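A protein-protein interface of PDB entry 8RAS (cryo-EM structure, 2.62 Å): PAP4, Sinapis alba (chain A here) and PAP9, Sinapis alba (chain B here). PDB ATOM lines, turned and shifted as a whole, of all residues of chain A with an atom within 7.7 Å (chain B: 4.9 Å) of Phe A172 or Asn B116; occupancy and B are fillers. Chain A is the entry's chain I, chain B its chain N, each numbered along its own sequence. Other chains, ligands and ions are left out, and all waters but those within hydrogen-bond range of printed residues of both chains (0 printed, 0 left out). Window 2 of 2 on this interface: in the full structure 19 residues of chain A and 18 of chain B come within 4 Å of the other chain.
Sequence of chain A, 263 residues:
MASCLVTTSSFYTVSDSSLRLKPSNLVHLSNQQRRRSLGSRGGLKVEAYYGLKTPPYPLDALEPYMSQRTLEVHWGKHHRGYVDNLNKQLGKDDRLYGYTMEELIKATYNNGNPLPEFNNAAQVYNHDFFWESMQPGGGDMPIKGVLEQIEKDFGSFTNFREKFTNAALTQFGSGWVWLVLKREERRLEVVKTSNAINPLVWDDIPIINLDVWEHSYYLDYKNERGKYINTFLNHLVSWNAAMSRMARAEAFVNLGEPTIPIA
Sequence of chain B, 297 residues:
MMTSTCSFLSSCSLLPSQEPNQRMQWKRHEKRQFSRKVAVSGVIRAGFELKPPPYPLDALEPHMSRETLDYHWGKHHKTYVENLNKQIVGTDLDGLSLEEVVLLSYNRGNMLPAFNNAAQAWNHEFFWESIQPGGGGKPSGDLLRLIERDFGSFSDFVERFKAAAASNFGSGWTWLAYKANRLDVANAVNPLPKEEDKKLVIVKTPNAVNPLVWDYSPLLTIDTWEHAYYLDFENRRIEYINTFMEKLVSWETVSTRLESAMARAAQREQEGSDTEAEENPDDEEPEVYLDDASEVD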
ATOM      1  N   ALA A 167       8.944 -30.676   1.256  1.00  0.00           N
ATOM      2  CA  ALA A 167      10.250 -30.554   0.621  1.00  0.00           C
ATOM      3  C   ALA A 167      10.833 -29.162   0.824  1.00  0.00           C
ATOM      4  O   ALA A 167      12.027 -29.013   1.105  1.00  0.00           O
ATOM      5  CB  ALA A 167      10.143 -30.882  -0.868  1.00  0.00           C
ATOM      6  N   ALA A 168      10.001 -28.127   0.689  1.00  0.00           N
ATOM      7  CA  ALA A 168      10.467 -26.763   0.908  1.00  0.00           C
ATOM      8  C   ALA A 168      10.620 -26.451   2.392  1.00  0.00           C
ATOM      9  O   ALA A 168      11.543 -25.726   2.784  1.00  0.00           O
ATOM     10  CB  ALA A 168       9.510 -25.770   0.248  1.00  0.00           C
ATOM     11  N   LEU A 169       9.724 -26.980   3.227  1.00  0.00           N
ATOM     12  CA  LEU A 169       9.804 -26.721   4.662  1.00  0.00           C
ATOM     13  C   LEU A 169      11.066 -27.323   5.268  1.00  0.00           C
ATOM     14  O   LEU A 169      11.708 -26.701   6.122  1.00  0.00           O
ATOM     15  CB  LEU A 169       8.559 -27.265   5.363  1.00  0.00           C
ATOM     16  CG  LEU A 169       7.279 -26.443   5.199  1.00  0.00           C
ATOM     17  CD1 LEU A 169       6.071 -27.214   5.711  1.00  0.00           C
ATOM     18  CD2 LEU A 169       7.402 -25.103   5.907  1.00  0.00           C
ATOM     19  N   THR A 170      11.440 -28.525   4.840  1.00  0.00           N
ATOM     20  CA  THR A 170      12.602 -29.215   5.384  1.00  0.00           C
ATOM     21  C   THR A 170      13.892 -28.885   4.646  1.00  0.00           C
ATOM     22  O   THR A 170      14.933 -29.471   4.959  1.00  0.00           O
ATOM     23  CB  THR A 170      12.377 -30.731   5.365  1.00  0.00           C
ATOM     24  OG1 THR A 170      11.875 -31.127   4.083  1.00  0.00           O
ATOM     25  CG2 THR A 170      11.381 -31.134   6.440  1.00  0.00           C
ATOM     26  N   GLN A 171      13.854 -27.971   3.679  1.00  0.00           N
ATOM     27  CA  GLN A 171      15.054 -27.569   2.955  1.00  0.00           C
ATOM     28  C   GLN A 171      15.868 -26.631   3.838  1.00  0.00           C
ATOM     29  O   GLN A 171      15.462 -25.491   4.088  1.00  0.00           O
ATOM     30  CB  GLN A 171      14.684 -26.902   1.632  1.00  0.00           C
ATOM     31  CG  GLN A 171      15.870 -26.348   0.855  1.00  0.00           C
ATOM     32  CD  GLN A 171      16.949 -27.384   0.598  1.00  0.00           C
ATOM     33  OE1 GLN A 171      16.660 -28.554   0.352  1.00  0.00           O
ATOM     34  NE2 GLN A 171      18.205 -26.953   0.649  1.00  0.00           N
ATOM     35  N   PHE A 172      17.016 -27.108   4.311  1.00  0.00           N
ATOM     36  CA  PHE A 172      17.874 -26.336   5.198  1.00  0.00           C
ATOM     37  C   PHE A 172      18.810 -25.486   4.346  1.00  0.00           C
ATOM     38  O   PHE A 172      19.572 -26.019   3.532  1.00  0.00           O
ATOM     39  CB  PHE A 172      18.670 -27.265   6.116  1.00  0.00           C
ATOM     40  CG  PHE A 172      19.527 -26.548   7.130  1.00  0.00           C
ATOM     41  CD1 PHE A 172      20.506 -27.233   7.825  1.00  0.00           C
ATOM     42  CD2 PHE A 172      19.314 -25.212   7.435  1.00  0.00           C
ATOM     43  CE1 PHE A 172      21.289 -26.591   8.766  1.00  0.00           C
ATOM     44  CE2 PHE A 172      20.090 -24.568   8.375  1.00  0.00           C
ATOM     45  CZ  PHE A 172      21.077 -25.258   9.042  1.00  0.00           C
ATOM     46  N   GLY A 173      18.755 -24.172   4.534  1.00  0.00           N
ATOM     47  CA  GLY A 173      19.622 -23.268   3.809  1.00  0.00           C
ATOM     48  C   GLY A 173      19.088 -22.914   2.438  1.00  0.00           C
ATOM     49  O   GLY A 173      17.974 -23.269   2.041  1.00  0.00           O
ATOM     50  N   SER A 174      19.918 -22.185   1.697  1.00  0.00           N
ATOM     51  CA  SER A 174      19.548 -21.759   0.355  1.00  0.00           C
ATOM     52  C   SER A 174      19.520 -22.952  -0.591  1.00  0.00           C
ATOM     53  O   SER A 174      20.456 -23.758  -0.621  1.00  0.00           O
ATOM     54  CB  SER A 174      20.528 -20.705  -0.151  1.00  0.00           C
ATOM     55  OG  SER A 174      21.866 -21.123   0.053  1.00  0.00           O
ATOM     56  N   GLY A 175      18.451 -23.062  -1.364  1.00  0.00           N
ATOM     57  CA  GLY A 175      18.319 -24.170  -2.282  1.00  0.00           C
ATOM     58  C   GLY A 175      17.119 -24.000  -3.184  1.00  0.00           C
ATOM     59  O   GLY A 175      16.604 -22.895  -3.360  1.00  0.00           O
ATOM     60  N   LYS A 192      13.992 -31.969  -3.520  1.00  0.00           N
ATOM     61  CA  LYS A 192      14.609 -30.821  -2.872  1.00  0.00           C
ATOM     62  C   LYS A 192      16.098 -30.808  -3.190  1.00  0.00           C
ATOM     63  O   LYS A 192      16.750 -31.856  -3.201  1.00  0.00           O
ATOM     64  CB  LYS A 192      14.395 -30.858  -1.356  1.00  0.00           C
ATOM     65  CG  LYS A 192      14.857 -32.145  -0.692  1.00  0.00           C
ATOM     66  CD  LYS A 192      14.935 -31.993   0.817  1.00  0.00           C
ATOM     67  CE  LYS A 192      13.550 -31.960   1.437  1.00  0.00           C
ATOM     68  NZ  LYS A 192      12.646 -32.974   0.828  1.00  0.00           N
ATOM     69  N   THR A 193      16.631 -29.620  -3.464  1.00  0.00           N
ATOM     70  CA  THR A 193      18.019 -29.489  -3.878  1.00  0.00           C
ATOM     71  C   THR A 193      18.607 -28.222  -3.273  1.00  0.00           C
ATOM     72  O   THR A 193      17.909 -27.220  -3.097  1.00  0.00           O
ATOM     73  CB  THR A 193      18.131 -29.467  -5.410  1.00  0.00           C
ATOM     74  OG1 THR A 193      17.567 -30.670  -5.944  1.00  0.00           O
ATOM     75  CG2 THR A 193      19.578 -29.402  -5.830  1.00  0.00           C
ATOM     76  N   SER A 194      19.899 -28.275  -2.957  1.00  0.00           N
ATOM     77  CA  SER A 194      20.597 -27.190  -2.285  1.00  0.00           C
ATOM     78  C   SER A 194      21.516 -26.448  -3.249  1.00  0.00           C
ATOM     79  O   SER A 194      22.010 -27.017  -4.228  1.00  0.00           O
ATOM     80  CB  SER A 194      21.416 -27.718  -1.104  1.00  0.00           C
ATOM     81  OG  SER A 194      22.726 -28.068  -1.515  1.00  0.00           O
ATOM     82  N   ASN A 195      21.730 -25.171  -2.954  1.00  0.00           N
ATOM     83  CA  ASN A 195      22.667 -24.284  -3.670  1.00  0.00           C
ATOM     84  C   ASN A 195      22.170 -24.125  -5.110  1.00  0.00           C
ATOM     85  O   ASN A 195      20.964 -23.941  -5.329  1.00  0.00           O
ATOM     86  CB  ASN A 195      24.081 -24.807  -3.532  1.00  0.00           C
ATOM     87  CG  ASN A 195      24.800 -24.228  -2.332  1.00  0.00           C
ATOM     88  OD1 ASN A 195      24.172 -23.697  -1.417  1.00  0.00           O
ATOM     89  ND2 ASN A 195      26.124 -24.322  -2.332  1.00  0.00           N
ATOM     90  N   VAL A 212      13.696 -21.236  -2.684  1.00  0.00           N
ATOM     91  CA  VAL A 212      13.702 -21.108  -1.233  1.00  0.00           C
ATOM     92  C   VAL A 212      14.969 -20.430  -0.734  1.00  0.00           C
ATOM     93  O   VAL A 212      15.268 -20.487   0.463  1.00  0.00           O
ATOM     94  CB  VAL A 212      13.494 -22.466  -0.544  1.00  0.00           C
ATOM     95  CG1 VAL A 212      12.080 -22.971  -0.788  1.00  0.00           C
ATOM     96  CG2 VAL A 212      14.514 -23.474  -1.027  1.00  0.00           C
ATOM     97  N   ARG A 225       8.868 -18.744   6.205  1.00  0.00           N
ATOM     98  CA  ARG A 225       8.887 -19.430   4.917  1.00  0.00           C
ATOM     99  C   ARG A 225       7.671 -20.328   4.737  1.00  0.00           C
ATOM    100  O   ARG A 225       7.269 -20.601   3.601  1.00  0.00           O
ATOM    101  CB  ARG A 225      10.176 -20.243   4.779  1.00  0.00           C
ATOM    102  CG  ARG A 225      10.411 -20.823   3.394  1.00  0.00           C
ATOM    103  CD  ARG A 225      11.293 -22.060   3.455  1.00  0.00           C
ATOM    104  NE  ARG A 225      12.697 -21.737   3.241  1.00  0.00           N
ATOM    105  CZ  ARG A 225      13.679 -22.628   3.237  1.00  0.00           C
ATOM    106  NH1 ARG A 225      13.445 -23.914   3.436  1.00  0.00           N
ATOM    107  NH2 ARG A 225      14.927 -22.219   3.030  1.00  0.00           N
ATOM    108  N   MET B 111      24.990 -36.630   9.826  1.00  0.00           N
ATOM    109  CA  MET B 111      24.468 -35.753  10.864  1.00  0.00           C
ATOM    110  C   MET B 111      23.112 -36.233  11.366  1.00  0.00           C
ATOM    111  O   MET B 111      22.233 -36.607  10.584  1.00  0.00           O
ATOM    112  CB  MET B 111      24.356 -34.325  10.328  1.00  0.00           C
ATOM    113  CG  MET B 111      25.677 -33.740   9.853  1.00  0.00           C
ATOM    114  SD  MET B 111      25.506 -32.698   8.390  1.00  0.00           S
ATOM    115  CE  MET B 111      23.882 -31.990   8.658  1.00  0.00           C
ATOM    116  N   LEU B 112      22.951 -36.220  12.686  1.00  0.00           N
ATOM    117  CA  LEU B 112      21.679 -36.546  13.302  1.00  0.00           C
ATOM    118  C   LEU B 112      20.676 -35.422  13.050  1.00  0.00           C
ATOM    119  O   LEU B 112      21.063 -34.291  12.746  1.00  0.00           O
ATOM    120  CB  LEU B 112      21.865 -36.774  14.800  1.00  0.00           C
ATOM    121  CG  LEU B 112      22.435 -38.135  15.204  1.00  0.00           C
ATOM    122  CD1 LEU B 112      22.708 -38.183  16.699  1.00  0.00           C
ATOM    123  CD2 LEU B 112      21.493 -39.257  14.789  1.00  0.00           C
ATOM    124  N   PRO B 113      19.375 -35.711  13.157  1.00  0.00           N
ATOM    125  CA  PRO B 113      18.374 -34.660  12.899  1.00  0.00           C
ATOM    126  C   PRO B 113      18.508 -33.451  13.808  1.00  0.00           C
ATOM    127  O   PRO B 113      18.114 -32.347  13.413  1.00  0.00           O
ATOM    128  CB  PRO B 113      17.040 -35.388  13.121  1.00  0.00           C
ATOM    129  CG  PRO B 113      17.348 -36.821  12.871  1.00  0.00           C
ATOM    130  CD  PRO B 113      18.746 -37.026  13.375  1.00  0.00           C
ATOM    131  N   ALA B 114      19.051 -33.621  15.011  1.00  0.00           N
ATOM    132  CA  ALA B 114      19.218 -32.512  15.941  1.00  0.00           C
ATOM    133  C   ALA B 114      20.482 -31.701  15.685  1.00  0.00           C
ATOM    134  O   ALA B 114      20.711 -30.708  16.384  1.00  0.00           O
ATOM    135  CB  ALA B 114      19.225 -33.031  17.381  1.00  0.00           C
ATOM    136  N   PHE B 115      21.308 -32.098  14.712  1.00  0.00           N
ATOM    137  CA  PHE B 115      22.544 -31.368  14.446  1.00  0.00           C
ATOM    138  C   PHE B 115      22.265 -29.958  13.946  1.00  0.00           C
ATOM    139  O   PHE B 115      22.965 -29.010  14.320  1.00  0.00           O
ATOM    140  CB  PHE B 115      23.401 -32.128  13.435  1.00  0.00           C
ATOM    141  CG  PHE B 115      24.690 -31.435  13.092  1.00  0.00           C
ATOM    142  CD1 PHE B 115      25.770 -31.485  13.955  1.00  0.00           C
ATOM    143  CD2 PHE B 115      24.820 -30.733  11.906  1.00  0.00           C
ATOM    144  CE1 PHE B 115      26.956 -30.849  13.643  1.00  0.00           C
ATOM    145  CE2 PHE B 115      26.004 -30.094  11.588  1.00  0.00           C
ATOM    146  CZ  PHE B 115      27.071 -30.152  12.458  1.00  0.00           C
ATOM    147  N   ASN B 116      21.249 -29.801  13.095  1.00  0.00           N
ATOM    148  CA  ASN B 116      21.010 -28.513  12.453  1.00  0.00           C
ATOM    149  C   ASN B 116      20.699 -27.431  13.480  1.00  0.00           C
ATOM    150  O   ASN B 116      21.340 -26.373  13.496  1.00  0.00           O
ATOM    151  CB  ASN B 116      19.868 -28.645  11.445  1.00  0.00           C
ATOM    152  CG  ASN B 116      20.247 -29.487  10.244  1.00  0.00           C
ATOM    153  OD1 ASN B 116      21.409 -29.522   9.837  1.00  0.00           O
ATOM    154  ND2 ASN B 116      19.267 -30.173   9.669  1.00  0.00           N
ATOM    155  N   ASN B 117      19.726 -27.689  14.356  1.00  0.00           N
ATOM    156  CA  ASN B 117      19.297 -26.673  15.314  1.00  0.00           C
ATOM    157  C   ASN B 117      20.404 -26.343  16.308  1.00  0.00           C
ATOM    158  O   ASN B 117      20.663 -25.168  16.593  1.00  0.00           O
ATOM    159  CB  ASN B 117      18.039 -27.145  16.044  1.00  0.00           C
ATOM    160  CG  ASN B 117      16.805 -27.103  15.164  1.00  0.00           C
ATOM    161  OD1 ASN B 117      16.560 -26.118  14.467  1.00  0.00           O
ATOM    162  ND2 ASN B 117      16.022 -28.175  15.190  1.00  0.00           N
ATOM    163  N   ALA B 118      21.070 -27.368  16.845  1.00  0.00           N
ATOM    164  CA  ALA B 118      22.126 -27.131  17.824  1.00  0.00           C
ATOM    165  C   ALA B 118      23.295 -26.375  17.206  1.00  0.00           C
ATOM    166  O   ALA B 118      23.830 -25.438  17.813  1.00  0.00           O
ATOM    167  CB  ALA B 118      22.600 -28.457  18.417  1.00  0.00           C
ATOM    168  N   ALA B 119      23.706 -26.767  15.998  1.00  0.00           N
ATOM    169  CA  ALA B 119      24.811 -26.085  15.337  1.00  0.00           C
ATOM    170  C   ALA B 119      24.453 -24.643  15.002  1.00  0.00           C
ATOM    171  O   ALA B 119      25.280 -23.740  15.171  1.00  0.00           O
ATOM    172  CB  ALA B 119      25.219 -26.849  14.079  1.00  0.00           C
ATOM    173  N   GLN B 120      23.225 -24.405  14.531  1.00  0.00           N
ATOM    174  CA  GLN B 120      22.807 -23.039  14.236  1.00  0.00           C
ATOM    175  C   GLN B 120      22.769 -22.191  15.500  1.00  0.00           C
ATOM    176  O   GLN B 120      23.185 -21.028  15.487  1.00  0.00           O
ATOM    177  CB  GLN B 120      21.443 -23.041  13.547  1.00  0.00           C
ATOM    178  CG  GLN B 120      21.511 -23.090  12.027  1.00  0.00           C
ATOM    179  CD  GLN B 120      22.129 -21.841  11.423  1.00  0.00           C
ATOM    180  OE1 GLN B 120      23.351 -21.707  11.355  1.00  0.00           O
ATOM    181  NE2 GLN B 120      21.284 -20.921  10.974  1.00  0.00           N
ATOM    182  N   ALA B 121      22.275 -22.759  16.605  1.00  0.00           N
ATOM    183  CA  ALA B 121      22.250 -22.022  17.863  1.00  0.00           C
ATOM    184  C   ALA B 121      23.660 -21.691  18.338  1.00  0.00           C
ATOM    185  O   ALA B 121      23.923 -20.570  18.787  1.00  0.00           O
ATOM    186  CB  ALA B 121      21.498 -22.822  18.925  1.00  0.00           C
ATOM    187  N   ASN B 207      25.705 -23.649   5.522  1.00  0.00           N
ATOM    188  CA  ASN B 207      24.571 -23.916   6.413  1.00  0.00           C
ATOM    189  C   ASN B 207      25.046 -23.790   7.856  1.00  0.00           C
ATOM    190  O   ASN B 207      25.538 -22.712   8.229  1.00  0.00           O
ATOM    191  CB  ASN B 207      23.947 -25.260   6.030  1.00  0.00           C
ATOM    192  CG  ASN B 207      23.742 -25.402   4.536  1.00  0.00           C
ATOM    193  OD1 ASN B 207      23.488 -24.420   3.838  1.00  0.00           O
ATOM    194  ND2 ASN B 207      23.852 -26.627   4.037  1.00  0.00           N
ATOM    195  N   ALA B 208      24.928 -24.823   8.687  1.00  0.00           N
ATOM    196  CA  ALA B 208      25.232 -24.729  10.108  1.00  0.00           C
ATOM    197  C   ALA B 208      26.573 -25.350  10.476  1.00  0.00           C
ATOM    198  O   ALA B 208      26.850 -25.537  11.666  1.00  0.00           O
ATOM    199  CB  ALA B 208      24.118 -25.382  10.926  1.00  0.00           C
ATOM    200  N   TRP B 225      24.950 -15.866   5.816  1.00  0.00           N
ATOM    201  CA  TRP B 225      23.541 -16.105   5.539  1.00  0.00           C
ATOM    202  C   TRP B 225      22.862 -14.800   5.155  1.00  0.00           C
ATOM    203  O   TRP B 225      23.077 -13.760   5.784  1.00  0.00           O
ATOM    204  CB  TRP B 225      22.850 -16.704   6.763  1.00  0.00           C
ATOM    205  CG  TRP B 225      23.025 -18.177   6.924  1.00  0.00           C
ATOM    206  CD1 TRP B 225      24.194 -18.850   7.114  1.00  0.00           C
ATOM    207  CD2 TRP B 225      21.988 -19.164   6.924  1.00  0.00           C
ATOM    208  NE1 TRP B 225      23.952 -20.197   7.226  1.00  0.00           N
ATOM    209  CE2 TRP B 225      22.604 -20.416   7.114  1.00  0.00           C
ATOM    210  CE3 TRP B 225      20.599 -19.110   6.779  1.00  0.00           C
ATOM    211  CZ2 TRP B 225      21.879 -21.604   7.162  1.00  0.00           C
ATOM    212  CZ3 TRP B 225      19.882 -20.289   6.828  1.00  0.00           C
ATOM    213  CH2 TRP B 225      20.522 -21.518   7.017  1.00  0.00           C
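The backbone carbonyl oxygen (O) of Asn B207 is in hydrogen-bond range of the indole nitrogen (NE1) of Trp B225 (3.1 Å).
The guanidinium group of Arg A225 lies within hydrogen-bond range of the backbone carbonyl oxygen of Gly A173.
Among the printed residues, merely in contact across the chains: Phe A172 with Asn B116 (3.1 Å), Phe A172 with Trp B225 (3.4 Å), Phe A172 with Ala B208 (3.6 Å), Phe A172 with Gln B120 (3.7 Å) and Gly A173 with Trp B225 (3.8 Å).
Of chain A, only Phe A172 comes within 4 Å of Asn B116.
Printed residues of chain B within 4 Å of Gly A173: Trp B225 (3.8 Å).
Of the printed residues of chain A, Ala B208 touches Phe A172 (3.6 Å).
Printed residues of chain A within 4 Å of Trp B225: Phe A172 (3.4 Å) and Gly A173 (3.8 Å).
The nearest printed residue of chain A that does not touch Ala B208 is Gly A173 (7.4 Å).
Printed residues of chain B that touch a printed residue of chain A: Asn B116, Gln B120, Ala B208 and Trp B225.
Of the 15 printed residues of chain A, 2 touch a printed residue of chain B.
Hydrophobic or aromatic side chains of chain A that line the printed part of chain B: Phe A172.
Among the printed residues, 5 pairs touch across the chains.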
